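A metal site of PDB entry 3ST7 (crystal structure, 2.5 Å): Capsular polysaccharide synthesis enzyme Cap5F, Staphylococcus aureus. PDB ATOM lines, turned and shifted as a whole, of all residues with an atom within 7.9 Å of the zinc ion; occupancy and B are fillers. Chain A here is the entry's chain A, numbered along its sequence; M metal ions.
The zinc ion is bound by the side-chain carboxylate of Glu 295, a ring nitrogen (NE2) of His 290 and a ring nitrogen (NE2) of His 337. The zinc ion has three donor atoms within binding distance. Slightly farther from the zinc ion lies the side-chain carboxylate (OE2) of Glu 295 (2.8 Å).
O of Glu 295 is in hydrogen-bond range of N of Ile 331, 2.8 Å away. The backbone carbonyl oxygen (O) of Asp 363 sits at hydrogen-bond distance from a ring nitrogen (ND1) of His 290, 2.8 Å away. The backbone NH (N) of His 337 sits at hydrogen-bond distance from the backbone carbonyl oxygen (O) of His 288, at 3.1 Å. The backbone carbonyl oxygen (O) of Tyr 335 sits at hydrogen-bond distance from a ring nitrogen (ND1) of His 337. O of His 337 lies within hydrogen-bond range of N of Asn 287, at 2.7 Å. N of His 288 is in hydrogen-bond range of OG1 of Thr 336, at 3.3 Å.
Merely in contact with the zinc ion: His 288 (2.9 Å). The nearest printed residue that does not touch the zinc ion is Ile 331 (4.6 Å).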
ATOM      1  N   GLY A 286     -33.620 -15.959   8.225  1.00  0.00           N
ATOM      2  CA  GLY A 286     -32.906 -15.207   9.242  1.00  0.00           C
ATOM      3  C   GLY A 286     -33.564 -15.353  10.595  1.00  0.00           C
ATOM      4  O   GLY A 286     -33.675 -16.465  11.124  1.00  0.00           O
ATOM      5  N   ASN A 287     -34.032 -14.222  11.129  1.00  0.00           N
ATOM      6  CA  ASN A 287     -34.535 -14.117  12.501  1.00  0.00           C
ATOM      7  C   ASN A 287     -33.468 -14.617  13.482  1.00  0.00           C
ATOM      8  O   ASN A 287     -33.728 -15.484  14.326  1.00  0.00           O
ATOM      9  CB  ASN A 287     -35.887 -14.849  12.688  1.00  0.00           C
ATOM     10  CG  ASN A 287     -37.074 -14.100  12.077  1.00  0.00           C
ATOM     11  OD1 ASN A 287     -37.214 -12.874  12.205  1.00  0.00           O
ATOM     12  ND2 ASN A 287     -37.961 -14.847  11.435  1.00  0.00           N
ATOM     13  N   HIS A 288     -32.275 -14.056  13.367  1.00  0.00           N
ATOM     14  CA  HIS A 288     -31.163 -14.403  14.238  1.00  0.00           C
ATOM     15  C   HIS A 288     -30.219 -13.190  14.409  1.00  0.00           C
ATOM     16  O   HIS A 288     -30.265 -12.271  13.590  1.00  0.00           O
ATOM     17  CB  HIS A 288     -30.414 -15.649  13.716  1.00  0.00           C
ATOM     18  CG  HIS A 288     -29.835 -15.504  12.339  1.00  0.00           C
ATOM     19  ND1 HIS A 288     -29.852 -16.527  11.415  1.00  0.00           N
ATOM     20  CD2 HIS A 288     -29.205 -14.472  11.720  1.00  0.00           C
ATOM     21  CE1 HIS A 288     -29.259 -16.138  10.298  1.00  0.00           C
ATOM     22  NE2 HIS A 288     -28.847 -14.891  10.457  1.00  0.00           N
ATOM     23  N   TRP A 289     -29.413 -13.183  15.470  1.00  0.00           N
ATOM     24  CA  TRP A 289     -28.389 -12.155  15.616  1.00  0.00           C
ATOM     25  C   TRP A 289     -27.022 -12.776  15.868  1.00  0.00           C
ATOM     26  O   TRP A 289     -26.915 -13.978  16.100  1.00  0.00           O
ATOM     27  CB  TRP A 289     -28.718 -11.163  16.723  1.00  0.00           C
ATOM     28  CG  TRP A 289     -28.893 -11.771  18.088  1.00  0.00           C
ATOM     29  CD1 TRP A 289     -29.992 -12.410  18.566  1.00  0.00           C
ATOM     30  CD2 TRP A 289     -27.934 -11.763  19.154  1.00  0.00           C
ATOM     31  NE1 TRP A 289     -29.790 -12.801  19.860  1.00  0.00           N
ATOM     32  CE2 TRP A 289     -28.533 -12.426  20.252  1.00  0.00           C
ATOM     33  CE3 TRP A 289     -26.637 -11.278  19.292  1.00  0.00           C
ATOM     34  CZ2 TRP A 289     -27.880 -12.620  21.469  1.00  0.00           C
ATOM     35  CZ3 TRP A 289     -25.972 -11.466  20.505  1.00  0.00           C
ATOM     36  CH2 TRP A 289     -26.600 -12.135  21.574  1.00  0.00           C
ATOM     37  N   HIS A 290     -25.989 -11.935  15.816  1.00  0.00           N
ATOM     38  CA  HIS A 290     -24.627 -12.385  16.076  1.00  0.00           C
ATOM     39  C   HIS A 290     -23.931 -11.457  17.062  1.00  0.00           C
ATOM     40  O   HIS A 290     -24.281 -10.288  17.147  1.00  0.00           O
ATOM     41  CB  HIS A 290     -23.804 -12.411  14.772  1.00  0.00           C
ATOM     42  CG  HIS A 290     -24.569 -12.848  13.570  1.00  0.00           C
ATOM     43  ND1 HIS A 290     -24.877 -14.166  13.320  1.00  0.00           N
ATOM     44  CD2 HIS A 290     -25.090 -12.135  12.541  1.00  0.00           C
ATOM     45  CE1 HIS A 290     -25.573 -14.251  12.205  1.00  0.00           C
ATOM     46  NE2 HIS A 290     -25.719 -13.029  11.711  1.00  0.00           N
ATOM     47  N   LYS A 293     -20.065 -11.949  14.079  1.00  0.00           N
ATOM     48  CA  LYS A 293     -20.326 -12.197  12.690  1.00  0.00           C
ATOM     49  C   LYS A 293     -21.105 -11.012  12.170  1.00  0.00           C
ATOM     50  O   LYS A 293     -22.039 -10.581  12.834  1.00  0.00           O
ATOM     51  CB  LYS A 293     -21.137 -13.464  12.505  1.00  0.00           C
ATOM     52  CG  LYS A 293     -21.166 -13.948  11.038  1.00  0.00           C
ATOM     53  CD  LYS A 293     -22.201 -15.042  10.765  1.00  0.00           C
ATOM     54  CE  LYS A 293     -21.943 -16.353  11.520  1.00  0.00           C
ATOM     55  NZ  LYS A 293     -20.542 -16.857  11.414  1.00  0.00           N
ATOM     56  N   ASN A 294     -20.722 -10.491  11.008  1.00  0.00           N
ATOM     57  CA  ASN A 294     -21.516  -9.490  10.293  1.00  0.00           C
ATOM     58  C   ASN A 294     -21.496  -9.689   8.781  1.00  0.00           C
ATOM     59  O   ASN A 294     -20.610 -10.355   8.245  1.00  0.00           O
ATOM     60  CB  ASN A 294     -21.121  -8.057  10.645  1.00  0.00           C
ATOM     61  CG  ASN A 294     -19.741  -7.683  10.129  1.00  0.00           C
ATOM     62  OD1 ASN A 294     -18.764  -7.685  10.889  1.00  0.00           O
ATOM     63  ND2 ASN A 294     -19.644  -7.317   8.864  1.00  0.00           N
ATOM     64  N   GLU A 295     -22.443  -9.077   8.109  1.00  0.00           N
ATOM     65  CA  GLU A 295     -22.719  -9.384   6.713  1.00  0.00           C
ATOM     66  C   GLU A 295     -23.008  -8.106   5.935  1.00  0.00           C
ATOM     67  O   GLU A 295     -23.280  -7.051   6.532  1.00  0.00           O
ATOM     68  CB  GLU A 295     -23.876 -10.382   6.630  1.00  0.00           C
ATOM     69  CG  GLU A 295     -23.666 -11.563   7.578  1.00  0.00           C
ATOM     70  CD  GLU A 295     -24.935 -12.176   8.126  1.00  0.00           C
ATOM     71  OE1 GLU A 295     -25.534 -11.669   9.120  1.00  0.00           O
ATOM     72  OE2 GLU A 295     -25.323 -13.220   7.573  1.00  0.00           O
ATOM     73  N   PHE A 297     -25.626  -7.468   2.756  1.00  0.00           N
ATOM     74  CA  PHE A 297     -26.613  -8.058   1.866  1.00  0.00           C
ATOM     75  C   PHE A 297     -26.751  -7.183   0.629  1.00  0.00           C
ATOM     76  O   PHE A 297     -26.880  -5.977   0.736  1.00  0.00           O
ATOM     77  CB  PHE A 297     -27.969  -8.222   2.534  1.00  0.00           C
ATOM     78  CG  PHE A 297     -28.035  -9.282   3.619  1.00  0.00           C
ATOM     79  CD1 PHE A 297     -26.957 -10.101   3.916  1.00  0.00           C
ATOM     80  CD2 PHE A 297     -29.206  -9.476   4.323  1.00  0.00           C
ATOM     81  CE1 PHE A 297     -27.048 -11.073   4.907  1.00  0.00           C
ATOM     82  CE2 PHE A 297     -29.307 -10.449   5.310  1.00  0.00           C
ATOM     83  CZ  PHE A 297     -28.216 -11.248   5.600  1.00  0.00           C
ATOM     84  N   ILE A 331     -25.142  -5.588   7.996  1.00  0.00           N
ATOM     85  CA  ILE A 331     -25.868  -6.248   9.078  1.00  0.00           C
ATOM     86  C   ILE A 331     -25.084  -6.098  10.392  1.00  0.00           C
ATOM     87  O   ILE A 331     -24.204  -6.894  10.679  1.00  0.00           O
ATOM     88  CB  ILE A 331     -26.114  -7.727   8.748  1.00  0.00           C
ATOM     89  CG1 ILE A 331     -26.592  -7.878   7.289  1.00  0.00           C
ATOM     90  CG2 ILE A 331     -27.058  -8.344   9.748  1.00  0.00           C
ATOM     91  CD1 ILE A 331     -27.995  -7.311   6.959  1.00  0.00           C
ATOM     92  N   PRO A 332     -25.391  -5.046  11.176  1.00  0.00           N
ATOM     93  CA  PRO A 332     -24.625  -4.772  12.398  1.00  0.00           C
ATOM     94  C   PRO A 332     -24.865  -5.812  13.495  1.00  0.00           C
ATOM     95  O   PRO A 332     -25.984  -6.302  13.653  1.00  0.00           O
ATOM     96  CB  PRO A 332     -25.151  -3.398  12.836  1.00  0.00           C
ATOM     97  CG  PRO A 332     -25.748  -2.820  11.593  1.00  0.00           C
ATOM     98  CD  PRO A 332     -26.361  -3.981  10.900  1.00  0.00           C
ATOM     99  N   TYR A 335     -27.968  -6.839  16.370  1.00  0.00           N
ATOM    100  CA  TYR A 335     -29.313  -6.687  15.816  1.00  0.00           C
ATOM    101  C   TYR A 335     -29.772  -8.025  15.266  1.00  0.00           C
ATOM    102  O   TYR A 335     -29.069  -8.645  14.461  1.00  0.00           O
ATOM    103  CB  TYR A 335     -29.362  -5.644  14.693  1.00  0.00           C
ATOM    104  CG  TYR A 335     -29.206  -4.210  15.145  1.00  0.00           C
ATOM    105  CD1 TYR A 335     -27.947  -3.669  15.354  1.00  0.00           C
ATOM    106  CD2 TYR A 335     -30.340  -3.389  15.325  1.00  0.00           C
ATOM    107  CE1 TYR A 335     -27.804  -2.342  15.754  1.00  0.00           C
ATOM    108  CE2 TYR A 335     -30.203  -2.059  15.737  1.00  0.00           C
ATOM    109  CZ  TYR A 335     -28.934  -1.539  15.950  1.00  0.00           C
ATOM    110  OH  TYR A 335     -28.752  -0.232  16.366  1.00  0.00           O
ATOM    111  N   THR A 336     -30.931  -8.488  15.706  1.00  0.00           N
ATOM    112  CA  THR A 336     -31.546  -9.614  15.036  1.00  0.00           C
ATOM    113  C   THR A 336     -32.059  -9.113  13.701  1.00  0.00           C
ATOM    114  O   THR A 336     -32.424  -7.938  13.565  1.00  0.00           O
ATOM    115  CB  THR A 336     -32.634 -10.289  15.880  1.00  0.00           C
ATOM    116  OG1 THR A 336     -33.093 -11.449  15.193  1.00  0.00           O
ATOM    117  CG2 THR A 336     -33.834  -9.327  16.177  1.00  0.00           C
ATOM    118  N   HIS A 337     -32.056  -9.969  12.693  1.00  0.00           N
ATOM    119  CA  HIS A 337     -32.415  -9.531  11.347  1.00  0.00           C
ATOM    120  C   HIS A 337     -33.100 -10.621  10.566  1.00  0.00           C
ATOM    121  O   HIS A 337     -32.909 -11.801  10.851  1.00  0.00           O
ATOM    122  CB  HIS A 337     -31.191  -9.046  10.591  1.00  0.00           C
ATOM    123  CG  HIS A 337     -30.004  -9.955  10.723  1.00  0.00           C
ATOM    124  ND1 HIS A 337     -29.181  -9.935  11.838  1.00  0.00           N
ATOM    125  CD2 HIS A 337     -29.503 -10.897   9.894  1.00  0.00           C
ATOM    126  CE1 HIS A 337     -28.208 -10.816  11.674  1.00  0.00           C
ATOM    127  NE2 HIS A 337     -28.377 -11.409  10.507  1.00  0.00           N
ATOM    128  N   ASN A 338     -33.922 -10.226   9.600  1.00  0.00           N
ATOM    129  CA  ASN A 338     -34.513 -11.188   8.678  1.00  0.00           C
ATOM    130  C   ASN A 338     -34.639 -10.597   7.295  1.00  0.00           C
ATOM    131  O   ASN A 338     -34.510  -9.399   7.127  1.00  0.00           O
ATOM    132  CB  ASN A 338     -35.813 -11.836   9.226  1.00  0.00           C
ATOM    133  CG  ASN A 338     -37.033 -10.912   9.180  1.00  0.00           C
ATOM    134  OD1 ASN A 338     -37.161 -10.039   8.332  1.00  0.00           O
ATOM    135  ND2 ASN A 338     -37.943 -11.126  10.105  1.00  0.00           N
ATOM    136  N   MET A 351     -24.508 -12.303  -0.413  1.00  0.00           N
ATOM    137  CA  MET A 351     -24.159 -12.052   0.978  1.00  0.00           C
ATOM    138  C   MET A 351     -22.684 -12.210   1.176  1.00  0.00           C
ATOM    139  O   MET A 351     -22.133 -13.272   0.919  1.00  0.00           O
ATOM    140  CB  MET A 351     -24.942 -12.996   1.895  1.00  0.00           C
ATOM    141  CG  MET A 351     -26.438 -13.019   1.605  1.00  0.00           C
ATOM    142  SD  MET A 351     -27.460 -14.054   2.906  1.00  0.00           S
ATOM    143  CE  MET A 351     -29.317 -13.436   2.561  1.00  0.00           C
ATOM    144  N   VAL A 353     -19.911 -12.190   4.159  1.00  0.00           N
ATOM    145  CA  VAL A 353     -19.870 -12.392   5.597  1.00  0.00           C
ATOM    146  C   VAL A 353     -18.401 -12.285   6.047  1.00  0.00           C
ATOM    147  O   VAL A 353     -17.509 -12.601   5.273  1.00  0.00           O
ATOM    148  CB  VAL A 353     -20.539 -13.731   6.018  1.00  0.00           C
ATOM    149  CG1 VAL A 353     -19.796 -14.886   5.451  1.00  0.00           C
ATOM    150  CG2 VAL A 353     -20.602 -13.860   7.522  1.00  0.00           C
ATOM    151  N   ASP A 363     -21.963 -18.643  16.299  1.00  0.00           N
ATOM    152  CA  ASP A 363     -22.221 -17.201  16.479  1.00  0.00           C
ATOM    153  C   ASP A 363     -23.511 -16.717  15.863  1.00  0.00           C
ATOM    154  O   ASP A 363     -23.580 -15.631  15.274  1.00  0.00           O
ATOM    155  CB  ASP A 363     -21.033 -16.306  16.084  1.00  0.00           C
ATOM    156  CG  ASP A 363     -21.128 -14.903  16.685  1.00  0.00           C
ATOM    157  OD1 ASP A 363     -21.829 -14.722  17.724  1.00  0.00           O
ATOM    158  OD2 ASP A 363     -20.493 -13.977  16.138  1.00  0.00           O
ATOM    159  N   THR A 364     -24.548 -17.525  15.986  1.00  0.00           N
ATOM    160  CA  THR A 364     -25.856 -17.070  15.548  1.00  0.00           C
ATOM    161  C   THR A 364     -26.924 -17.565  16.509  1.00  0.00           C
ATOM    162  O   THR A 364     -26.886 -18.708  16.943  1.00  0.00           O
ATOM    163  CB  THR A 364     -26.141 -17.276  13.997  1.00  0.00           C
ATOM    164  OG1 THR A 364     -27.160 -18.244  13.764  1.00  0.00           O
ATOM    165  CG2 THR A 364     -24.922 -17.640  13.223  1.00  0.00           C
HETATM  166 ZN    ZN M   1     -26.878 -12.896   9.852  1.00  0.00          ZN
